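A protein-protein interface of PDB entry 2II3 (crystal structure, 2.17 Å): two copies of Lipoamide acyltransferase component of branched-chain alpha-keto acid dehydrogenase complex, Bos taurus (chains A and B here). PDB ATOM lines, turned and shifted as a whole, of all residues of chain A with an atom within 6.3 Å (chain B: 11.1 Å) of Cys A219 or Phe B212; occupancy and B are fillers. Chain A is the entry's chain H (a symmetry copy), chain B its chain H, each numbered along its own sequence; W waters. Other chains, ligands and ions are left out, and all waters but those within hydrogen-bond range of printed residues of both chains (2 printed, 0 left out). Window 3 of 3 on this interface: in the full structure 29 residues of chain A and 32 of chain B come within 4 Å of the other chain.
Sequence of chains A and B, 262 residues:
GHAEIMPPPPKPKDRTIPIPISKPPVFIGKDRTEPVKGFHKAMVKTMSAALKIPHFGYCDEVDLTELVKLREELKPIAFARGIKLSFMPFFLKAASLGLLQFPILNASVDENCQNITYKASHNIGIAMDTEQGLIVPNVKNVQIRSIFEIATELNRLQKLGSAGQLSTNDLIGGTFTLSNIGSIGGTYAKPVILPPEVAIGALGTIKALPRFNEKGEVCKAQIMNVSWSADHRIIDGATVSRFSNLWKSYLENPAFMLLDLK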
ATOM      1  N   ALA A 208       8.995 -18.401  27.015  1.00  0.00           N
ATOM      2  CA  ALA A 208       9.808 -19.165  26.061  1.00  0.00           C
ATOM      3  C   ALA A 208       8.942 -19.433  24.854  1.00  0.00           C
ATOM      4  O   ALA A 208       7.912 -20.087  24.988  1.00  0.00           O
ATOM      5  CB  ALA A 208      10.251 -20.436  26.648  1.00  0.00           C
ATOM      6  N   LEU A 209       9.330 -18.895  23.691  1.00  0.00           N
ATOM      7  CA  LEU A 209       8.583 -19.132  22.417  1.00  0.00           C
ATOM      8  C   LEU A 209       9.511 -19.701  21.377  1.00  0.00           C
ATOM      9  O   LEU A 209      10.692 -19.374  21.375  1.00  0.00           O
ATOM     10  CB  LEU A 209       8.010 -17.802  21.862  1.00  0.00           C
ATOM     11  CG  LEU A 209       6.968 -17.134  22.749  1.00  0.00           C
ATOM     12  CD1 LEU A 209       6.550 -15.768  22.224  1.00  0.00           C
ATOM     13  CD2 LEU A 209       5.728 -17.983  22.977  1.00  0.00           C
ATOM     14  N   PRO A 210       8.970 -20.486  20.431  1.00  0.00           N
ATOM     15  CA  PRO A 210       9.835 -20.946  19.355  1.00  0.00           C
ATOM     16  C   PRO A 210      10.119 -19.788  18.369  1.00  0.00           C
ATOM     17  O   PRO A 210       9.172 -19.113  17.899  1.00  0.00           O
ATOM     18  CB  PRO A 210       9.028 -22.094  18.729  1.00  0.00           C
ATOM     19  CG  PRO A 210       7.836 -22.287  19.703  1.00  0.00           C
ATOM     20  CD  PRO A 210       7.599 -20.987  20.278  1.00  0.00           C
ATOM     21  N   ARG A 211      11.405 -19.518  18.112  1.00  0.00           N
ATOM     22  CA  ARG A 211      11.830 -18.379  17.272  1.00  0.00           C
ATOM     23  C   ARG A 211      13.009 -18.843  16.419  1.00  0.00           C
ATOM     24  O   ARG A 211      13.797 -19.699  16.857  1.00  0.00           O
ATOM     25  CB  ARG A 211      12.222 -17.168  18.113  1.00  0.00           C
ATOM     26  CG  ARG A 211      11.072 -16.355  18.793  1.00  0.00           C
ATOM     27  CD  ARG A 211      10.395 -15.401  17.827  1.00  0.00           C
ATOM     28  NE  ARG A 211       9.273 -14.607  18.345  1.00  0.00           N
ATOM     29  CZ  ARG A 211       8.048 -15.104  18.487  1.00  0.00           C
ATOM     30  NH1 ARG A 211       7.835 -16.385  18.211  1.00  0.00           N
ATOM     31  NH2 ARG A 211       7.042 -14.325  18.904  1.00  0.00           N
ATOM     32  N   PHE A 212      13.131 -18.295  15.208  1.00  0.00           N
ATOM     33  CA  PHE A 212      14.282 -18.608  14.358  1.00  0.00           C
ATOM     34  C   PHE A 212      15.597 -17.980  14.839  1.00  0.00           C
ATOM     35  O   PHE A 212      15.629 -16.814  15.295  1.00  0.00           O
ATOM     36  CB  PHE A 212      14.029 -18.249  12.898  1.00  0.00           C
ATOM     37  CG  PHE A 212      13.003 -19.108  12.239  1.00  0.00           C
ATOM     38  CD1 PHE A 212      13.205 -20.475  12.109  1.00  0.00           C
ATOM     39  CD2 PHE A 212      11.834 -18.558  11.763  1.00  0.00           C
ATOM     40  CE1 PHE A 212      12.278 -21.273  11.518  1.00  0.00           C
ATOM     41  CE2 PHE A 212      10.871 -19.365  11.139  1.00  0.00           C
ATOM     42  CZ  PHE A 212      11.087 -20.714  11.023  1.00  0.00           C
ATOM     43  N   ASN A 213      16.677 -18.755  14.735  1.00  0.00           N
ATOM     44  CA  ASN A 213      18.032 -18.144  14.830  1.00  0.00           C
ATOM     45  C   ASN A 213      18.515 -17.658  13.457  1.00  0.00           C
ATOM     46  O   ASN A 213      17.740 -17.679  12.482  1.00  0.00           O
ATOM     47  CB  ASN A 213      19.074 -19.031  15.568  1.00  0.00           C
ATOM     48  CG  ASN A 213      19.418 -20.333  14.837  1.00  0.00           C
ATOM     49  OD1 ASN A 213      19.020 -20.590  13.687  1.00  0.00           O
ATOM     50  ND2 ASN A 213      20.187 -21.175  15.519  1.00  0.00           N
ATOM     51  N   GLU A 217      17.193 -21.984  12.185  1.00  0.00           N
ATOM     52  CA  GLU A 217      16.824 -23.108  13.035  1.00  0.00           C
ATOM     53  C   GLU A 217      15.848 -22.628  14.119  1.00  0.00           C
ATOM     54  O   GLU A 217      15.985 -21.526  14.643  1.00  0.00           O
ATOM     55  CB  GLU A 217      18.067 -23.704  13.698  1.00  0.00           C
ATOM     56  CG  GLU A 217      19.061 -24.377  12.716  1.00  0.00           C
ATOM     57  CD  GLU A 217      20.439 -24.682  13.339  1.00  0.00           C
ATOM     58  OE1 GLU A 217      20.829 -24.007  14.335  1.00  0.00           O
ATOM     59  OE2 GLU A 217      21.138 -25.588  12.803  1.00  0.00           O
ATOM     60  N   VAL A 218      14.885 -23.482  14.452  1.00  0.00           N
ATOM     61  CA  VAL A 218      13.920 -23.219  15.492  1.00  0.00           C
ATOM     62  C   VAL A 218      14.592 -23.358  16.858  1.00  0.00           C
ATOM     63  O   VAL A 218      15.044 -24.432  17.227  1.00  0.00           O
ATOM     64  CB  VAL A 218      12.649 -24.112  15.353  1.00  0.00           C
ATOM     65  CG1 VAL A 218      11.577 -23.698  16.384  1.00  0.00           C
ATOM     66  CG2 VAL A 218      12.057 -23.982  13.973  1.00  0.00           C
ATOM     67  N   CYS A 219      14.632 -22.263  17.600  1.00  0.00           N
ATOM     68  CA  CYS A 219      15.267 -22.201  18.915  1.00  0.00           C
ATOM     69  C   CYS A 219      14.271 -21.757  19.970  1.00  0.00           C
ATOM     70  O   CYS A 219      13.252 -21.152  19.637  1.00  0.00           O
ATOM     71  CB  CYS A 219      16.427 -21.198  18.892  1.00  0.00           C
ATOM     72  SG  CYS A 219      17.611 -21.500  17.595  1.00  0.00           S
ATOM     73  N   LYS A 220      14.586 -22.023  21.239  1.00  0.00           N
ATOM     74  CA  LYS A 220      13.824 -21.491  22.389  1.00  0.00           C
ATOM     75  C   LYS A 220      14.349 -20.088  22.685  1.00  0.00           C
ATOM     76  O   LYS A 220      15.521 -19.921  23.032  1.00  0.00           O
ATOM     77  CB  LYS A 220      13.975 -22.399  23.626  1.00  0.00           C
ATOM     78  CG  LYS A 220      13.311 -21.897  24.902  1.00  0.00           C
ATOM     79  CD  LYS A 220      13.681 -22.825  26.104  1.00  0.00           C
ATOM     80  CE  LYS A 220      12.625 -23.918  26.292  1.00  0.00           C
ATOM     81  NZ  LYS A 220      12.706 -24.668  27.608  1.00  0.00           N
ATOM     82  N   ALA A 221      13.489 -19.084  22.517  1.00  0.00           N
ATOM     83  CA  ALA A 221      13.817 -17.724  22.807  1.00  0.00           C
ATOM     84  C   ALA A 221      12.930 -17.198  23.926  1.00  0.00           C
ATOM     85  O   ALA A 221      11.719 -17.500  23.998  1.00  0.00           O
ATOM     86  CB  ALA A 221      13.656 -16.855  21.546  1.00  0.00           C
ATOM     87  N   GLU B  61      -2.347 -13.894  26.050  1.00  0.00           N
ATOM     88  CA  GLU B  61      -2.683 -15.018  25.219  1.00  0.00           C
ATOM     89  C   GLU B  61      -3.090 -16.194  26.157  1.00  0.00           C
ATOM     90  O   GLU B  61      -2.620 -16.298  27.296  1.00  0.00           O
ATOM     91  CB  GLU B  61      -1.503 -15.336  24.243  1.00  0.00           C
ATOM     92  CG  GLU B  61      -0.535 -16.358  24.692  1.00  0.00           C
ATOM     93  CD  GLU B  61       0.397 -16.943  23.583  1.00  0.00           C
ATOM     94  OE1 GLU B  61       0.665 -16.301  22.521  1.00  0.00           O
ATOM     95  OE2 GLU B  61       0.870 -18.079  23.808  1.00  0.00           O
ATOM     96  N   ASP B  63      -4.033 -20.465  26.176  1.00  0.00           N
ATOM     97  CA  ASP B  63      -3.810 -21.704  25.435  1.00  0.00           C
ATOM     98  C   ASP B  63      -5.064 -22.548  25.545  1.00  0.00           C
ATOM     99  O   ASP B  63      -5.356 -23.116  26.623  1.00  0.00           O
ATOM    100  CB  ASP B  63      -2.601 -22.453  25.949  1.00  0.00           C
ATOM    101  CG  ASP B  63      -2.326 -23.707  25.165  1.00  0.00           C
ATOM    102  OD1 ASP B  63      -3.183 -24.119  24.363  1.00  0.00           O
ATOM    103  OD2 ASP B  63      -1.254 -24.305  25.347  1.00  0.00           O
ATOM    104  N   THR B  65      -5.902 -25.214  23.773  1.00  0.00           N
ATOM    105  CA  THR B  65      -5.774 -26.584  23.281  1.00  0.00           C
ATOM    106  C   THR B  65      -6.764 -27.561  23.938  1.00  0.00           C
ATOM    107  O   THR B  65      -7.468 -28.344  23.221  1.00  0.00           O
ATOM    108  CB  THR B  65      -4.327 -27.130  23.390  1.00  0.00           C
ATOM    109  OG1 THR B  65      -3.434 -26.196  22.793  1.00  0.00           O
ATOM    110  CG2 THR B  65      -4.193 -28.490  22.678  1.00  0.00           C
ATOM    111  N   ALA B 208      -3.910 -22.018  15.531  1.00  0.00           N
ATOM    112  CA  ALA B 208      -2.904 -23.045  15.833  1.00  0.00           C
ATOM    113  C   ALA B 208      -1.549 -22.410  15.641  1.00  0.00           C
ATOM    114  O   ALA B 208      -1.239 -21.977  14.535  1.00  0.00           O
ATOM    115  CB  ALA B 208      -3.046 -24.198  14.933  1.00  0.00           C
ATOM    116  N   LEU B 209      -0.762 -22.311  16.720  1.00  0.00           N
ATOM    117  CA  LEU B 209       0.622 -21.747  16.646  1.00  0.00           C
ATOM    118  C   LEU B 209       1.610 -22.745  17.186  1.00  0.00           C
ATOM    119  O   LEU B 209       1.275 -23.501  18.090  1.00  0.00           O
ATOM    120  CB  LEU B 209       0.735 -20.458  17.501  1.00  0.00           C
ATOM    121  CG  LEU B 209      -0.131 -19.298  17.029  1.00  0.00           C
ATOM    122  CD1 LEU B 209      -0.087 -18.115  17.984  1.00  0.00           C
ATOM    123  CD2 LEU B 209       0.204 -18.820  15.625  1.00  0.00           C
ATOM    124  N   PRO B 210       2.863 -22.697  16.704  1.00  0.00           N
ATOM    125  CA  PRO B 210       3.856 -23.576  17.302  1.00  0.00           C
ATOM    126  C   PRO B 210       4.269 -23.042  18.694  1.00  0.00           C
ATOM    127  O   PRO B 210       4.617 -21.846  18.832  1.00  0.00           O
ATOM    128  CB  PRO B 210       5.000 -23.553  16.276  1.00  0.00           C
ATOM    129  CG  PRO B 210       4.403 -22.787  15.066  1.00  0.00           C
ATOM    130  CD  PRO B 210       3.438 -21.877  15.630  1.00  0.00           C
ATOM    131  N   ARG B 211       4.169 -23.896  19.720  1.00  0.00           N
ATOM    132  CA  ARG B 211       4.429 -23.500  21.118  1.00  0.00           C
ATOM    133  C   ARG B 211       5.165 -24.651  21.802  1.00  0.00           C
ATOM    134  O   ARG B 211       4.941 -25.824  21.455  1.00  0.00           O
ATOM    135  CB  ARG B 211       3.142 -23.168  21.866  1.00  0.00           C
ATOM    136  CG  ARG B 211       2.430 -21.820  21.521  1.00  0.00           C
ATOM    137  CD  ARG B 211       3.076 -20.635  22.214  1.00  0.00           C
ATOM    138  NE  ARG B 211       2.513 -19.308  21.937  1.00  0.00           N
ATOM    139  CZ  ARG B 211       2.793 -18.627  20.830  1.00  0.00           C
ATOM    140  NH1 ARG B 211       3.560 -19.188  19.904  1.00  0.00           N
ATOM    141  NH2 ARG B 211       2.306 -17.393  20.649  1.00  0.00           N
ATOM    142  N   PHE B 212       6.040 -24.330  22.756  1.00  0.00           N
ATOM    143  CA  PHE B 212       6.720 -25.371  23.528  1.00  0.00           C
ATOM    144  C   PHE B 212       5.808 -26.097  24.528  1.00  0.00           C
ATOM    145  O   PHE B 212       4.953 -25.472  25.196  1.00  0.00           O
ATOM    146  CB  PHE B 212       7.961 -24.838  24.237  1.00  0.00           C
ATOM    147  CG  PHE B 212       9.067 -24.467  23.309  1.00  0.00           C
ATOM    148  CD1 PHE B 212       9.658 -25.424  22.496  1.00  0.00           C
ATOM    149  CD2 PHE B 212       9.508 -23.164  23.235  1.00  0.00           C
ATOM    150  CE1 PHE B 212      10.663 -25.101  21.641  1.00  0.00           C
ATOM    151  CE2 PHE B 212      10.552 -22.816  22.367  1.00  0.00           C
ATOM    152  CZ  PHE B 212      11.122 -23.774  21.568  1.00  0.00           C
ATOM    153  N   ASN B 213       5.996 -27.413  24.626  1.00  0.00           N
ATOM    154  CA  ASN B 213       5.434 -28.150  25.792  1.00  0.00           C
ATOM    155  C   ASN B 213       6.414 -28.142  26.974  1.00  0.00           C
ATOM    156  O   ASN B 213       7.451 -27.452  26.916  1.00  0.00           O
ATOM    157  CB  ASN B 213       4.903 -29.570  25.446  1.00  0.00           C
ATOM    158  CG  ASN B 213       5.991 -30.555  25.005  1.00  0.00           C
ATOM    159  OD1 ASN B 213       7.207 -30.293  25.064  1.00  0.00           O
ATOM    160  ND2 ASN B 213       5.545 -31.724  24.560  1.00  0.00           N
ATOM    161  N   GLU B 214       6.083 -28.876  28.039  1.00  0.00           N
ATOM    162  CA  GLU B 214       6.970 -28.961  29.218  1.00  0.00           C
ATOM    163  C   GLU B 214       8.256 -29.749  28.974  1.00  0.00           C
ATOM    164  O   GLU B 214       9.288 -29.466  29.577  1.00  0.00           O
ATOM    165  CB  GLU B 214       6.222 -29.473  30.458  1.00  0.00           C
ATOM    166  CG  GLU B 214       5.674 -28.314  31.290  1.00  0.00           C
ATOM    167  CD  GLU B 214       4.364 -28.648  31.975  1.00  0.00           C
ATOM    168  OE1 GLU B 214       4.302 -29.745  32.624  1.00  0.00           O
ATOM    169  OE2 GLU B 214       3.411 -27.806  31.851  1.00  0.00           O
ATOM    170  N   LYS B 215       8.203 -30.720  28.070  1.00  0.00           N
ATOM    171  CA  LYS B 215       9.429 -31.337  27.572  1.00  0.00           C
ATOM    172  C   LYS B 215      10.314 -30.392  26.718  1.00  0.00           C
ATOM    173  O   LYS B 215      11.460 -30.724  26.430  1.00  0.00           O
ATOM    174  CB  LYS B 215       9.101 -32.621  26.789  1.00  0.00           C
ATOM    175  CG  LYS B 215       8.631 -33.814  27.647  1.00  0.00           C
ATOM    176  CD  LYS B 215       9.237 -35.127  27.128  1.00  0.00           C
ATOM    177  CE  LYS B 215      10.678 -35.329  27.661  1.00  0.00           C
ATOM    178  NZ  LYS B 215      11.605 -36.042  26.736  1.00  0.00           N
ATOM    179  N   GLY B 216       9.788 -29.239  26.301  1.00  0.00           N
ATOM    180  CA  GLY B 216      10.535 -28.334  25.419  1.00  0.00           C
ATOM    181  C   GLY B 216      10.489 -28.791  23.973  1.00  0.00           C
ATOM    182  O   GLY B 216      11.415 -28.526  23.186  1.00  0.00           O
ATOM    183  N   GLU B 217       9.426 -29.525  23.642  1.00  0.00           N
ATOM    184  CA  GLU B 217       9.139 -29.959  22.282  1.00  0.00           C
ATOM    185  C   GLU B 217       8.152 -28.979  21.632  1.00  0.00           C
ATOM    186  O   GLU B 217       7.238 -28.482  22.286  1.00  0.00           O
ATOM    187  CB  GLU B 217       8.531 -31.364  22.289  1.00  0.00           C
ATOM    188  CG  GLU B 217       9.494 -32.479  22.769  1.00  0.00           C
ATOM    189  CD  GLU B 217       8.790 -33.818  23.076  1.00  0.00           C
ATOM    190  OE1 GLU B 217       7.561 -33.814  23.377  1.00  0.00           O
ATOM    191  OE2 GLU B 217       9.488 -34.870  23.042  1.00  0.00           O
ATOM    192  N   VAL B 218       8.342 -28.734  20.339  1.00  0.00           N
ATOM    193  CA  VAL B 218       7.473 -27.888  19.558  1.00  0.00           C
ATOM    194  C   VAL B 218       6.160 -28.620  19.283  1.00  0.00           C
ATOM    195  O   VAL B 218       6.143 -29.646  18.618  1.00  0.00           O
ATOM    196  CB  VAL B 218       8.164 -27.382  18.255  1.00  0.00           C
ATOM    197  CG1 VAL B 218       7.268 -26.359  17.525  1.00  0.00           C
ATOM    198  CG2 VAL B 218       9.479 -26.718  18.574  1.00  0.00           C
ATOM    199  N   CYS B 219       5.069 -28.067  19.787  1.00  0.00           N
ATOM    200  CA  CYS B 219       3.734 -28.647  19.657  1.00  0.00           C
ATOM    201  C   CYS B 219       2.790 -27.670  18.981  1.00  0.00           C
ATOM    202  O   CYS B 219       3.053 -26.467  18.973  1.00  0.00           O
ATOM    203  CB  CYS B 219       3.169 -28.987  21.042  1.00  0.00           C
ATOM    204  SG  CYS B 219       4.247 -30.012  22.023  1.00  0.00           S
ATOM    205  N   LYS B 220       1.677 -28.182  18.452  1.00  0.00           N
ATOM    206  CA  LYS B 220       0.571 -27.348  17.935  1.00  0.00           C
ATOM    207  C   LYS B 220      -0.316 -26.967  19.116  1.00  0.00           C
ATOM    208  O   LYS B 220      -0.909 -27.840  19.758  1.00  0.00           O
ATOM    209  CB  LYS B 220      -0.242 -28.104  16.865  1.00  0.00           C
ATOM    210  CG  LYS B 220      -1.470 -27.378  16.330  1.00  0.00           C
ATOM    211  CD  LYS B 220      -2.285 -28.319  15.384  1.00  0.00           C
ATOM    212  CE  LYS B 220      -1.856 -28.129  13.927  1.00  0.00           C
ATOM    213  NZ  LYS B 220      -2.788 -28.743  12.900  1.00  0.00           N
ATOM    214  N   ALA B 221      -0.382 -25.671  19.417  1.00  0.00           N
ATOM    215  CA  ALA B 221      -1.212 -25.157  20.460  1.00  0.00           C
ATOM    216  C   ALA B 221      -2.265 -24.223  19.878  1.00  0.00           C
ATOM    217  O   ALA B 221      -1.998 -23.434  18.947  1.00  0.00           O
ATOM    218  CB  ALA B 221      -0.359 -24.413  21.505  1.00  0.00           C
ATOM    219  N   GLN B 222      -3.468 -24.320  20.433  1.00  0.00           N
ATOM    220  CA  GLN B 222      -4.586 -23.500  19.966  1.00  0.00           C
ATOM    221  C   GLN B 222      -4.604 -22.252  20.836  1.00  0.00           C
ATOM    222  O   GLN B 222      -4.996 -22.321  21.989  1.00  0.00           O
ATOM    223  CB  GLN B 222      -5.918 -24.239  20.062  1.00  0.00           C
ATOM    224  CG  GLN B 222      -5.967 -25.611  19.369  1.00  0.00           C
ATOM    225  CD  GLN B 222      -5.998 -25.469  17.830  1.00  0.00           C
ATOM    226  OE1 GLN B 222      -5.669 -26.400  17.119  1.00  0.00           O
ATOM    227  NE2 GLN B 222      -6.380 -24.287  17.332  1.00  0.00           N
ATOM    228  N   ILE B 223      -4.175 -21.130  20.275  1.00  0.00           N
ATOM    229  CA  ILE B 223      -3.934 -19.884  21.040  1.00  0.00           C
ATOM    230  C   ILE B 223      -5.011 -18.848  20.712  1.00  0.00           C
ATOM    231  O   ILE B 223      -5.368 -18.682  19.560  1.00  0.00           O
ATOM    232  CB  ILE B 223      -2.511 -19.349  20.699  1.00  0.00           C
ATOM    233  CG1 ILE B 223      -1.419 -20.395  21.072  1.00  0.00           C
ATOM    234  CG2 ILE B 223      -2.233 -17.931  21.272  1.00  0.00           C
ATOM    235  CD1 ILE B 223      -1.425 -20.762  22.598  1.00  0.00           C
ATOM    236  N   GLU B 252      -7.755 -22.723  30.481  1.00  0.00           N
ATOM    237  CA  GLU B 252      -6.607 -23.625  30.211  1.00  0.00           C
ATOM    238  C   GLU B 252      -6.742 -24.983  30.919  1.00  0.00           C
ATOM    239  O   GLU B 252      -6.276 -26.021  30.399  1.00  0.00           O
ATOM    240  CB  GLU B 252      -5.249 -22.935  30.521  1.00  0.00           C
ATOM    241  CG  GLU B 252      -5.042 -21.702  29.692  1.00  0.00           C
ATOM    242  CD  GLU B 252      -3.631 -21.093  29.796  1.00  0.00           C
ATOM    243  OE1 GLU B 252      -2.913 -21.298  30.821  1.00  0.00           O
ATOM    244  OE2 GLU B 252      -3.238 -20.389  28.826  1.00  0.00           O
HETATM  245  O   HOH W   1       6.247 -19.872  16.997  1.00  0.00           O
HETATM  246  O   HOH W   2       6.163 -21.583  23.809  1.00  0.00           O
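The side-chain carboxylate (OE1) of Glu B61 lies within salt-bridge range of the guanidinium group (NH2) of Arg B211, 2.7 Å away.
O of Arg B211 sits at hydrogen-bond distance from N of Cys B219.
N of Leu A209 is in hydrogen-bond range of O of Ala A221 (2.8 Å).
The backbone NH (N) of Cys A219 is in hydrogen-bond range of the backbone carbonyl oxygen (O) of Arg A211 (2.8 Å).
The side-chain amide nitrogen (ND2) of Asn A213 lies within hydrogen-bond range of the side-chain sulfur (SG) of Cys A219, at 3.3 Å.
O of Glu A217 sits at hydrogen-bond distance from SG of Cys A219 (3.4 Å).
Phe B212 touches Ala A208.
Leu A209 touches Arg B211 (CD2 to NE, 3.6 Å).
C of Leu A209 touches CE2 of Phe B212, 3.4 Å away.
Pro B210 touches Pro A210 (O to CG, 3.4 Å).
CG of Pro A210 touches CA of Arg B211 (3.9 Å).
CE2 of Phe B212 touches N of Pro A210, 3.4 Å away.
Phe B212 touches Cys A219.
Lys A220 touches Phe B212.
Of the printed residues of chain B, Leu A209 touches Arg B211 and Phe B212.
Of chain B, only Pro B210 (3.4 Å), Arg B211 (3.9 Å) and Phe B212 (3.4 Å) come within 4 Å of Pro A210.
No residue of chain B comes within 4 Å of Asn A213.
No residue of chain B comes within 4 Å of Val A218.
No residue of chain B comes within 4 Å of Ala A221.
Of the printed residues of chain A, Pro B210 touches Pro A210 (3.4 Å).
Of the printed residues of chain A, Arg B211 touches Leu A209 and Pro A210.
Of the printed residues of chain A, Phe B212 touches Ala A208 (3.9 Å), Leu A209 (3.4 Å), Pro A210 (3.4 Å), Cys A219 (3.9 Å) and Lys A220 (3.5 Å).
The nearest printed residue of chain B that does not touch Cys A219 is Val B218 (6.8 Å).
The nearest printed residue of chain A that does not touch Pro B210 is Leu A209 (5.8 Å).
Hydrophobic or aromatic side chains of chain A that line the printed part of chain B: Leu A209 and Pro A210.
Of the 20 printed residues of chain B, 3 touch a printed residue of chain A.
Hydrophobic or aromatic side chains of chain B that line the printed part of chain A: Phe B212.
Along chain B the printed residues that touch a printed residue of chain A span positions 210 to 212.
Among the printed residues, 8 pairs touch across the chains.
Ala A208 touches Phe B212, but with the chains exchanged Phe A212 does not touch Ala B208 (12.8 Å).
Leu A209 touches Arg B211, but with the chains exchanged Arg A211 does not touch Leu B209 (8.1 Å).
Pro A210 touches Arg B211, but with the chains exchanged Arg A211 does not touch Pro B210 (6.4 Å).
Lys A220 touches Phe B212, but with the chains exchanged Phe A212 does not touch Lys B220 (14.1 Å).
Positions printed for both chains: 208, 209, 210, 211, 212, 213, 217, 218, 219, 220 and 221.
Water W2 bridges the backbone carbonyl oxygen of Ala A208 (2.6 Å) and the backbone NH of Phe B212 (2.9 Å).
Water W1 lies within hydrogen-bond range of the backbone carbonyl oxygen of Pro B210 and the backbone carbonyl oxygen of Pro A210.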
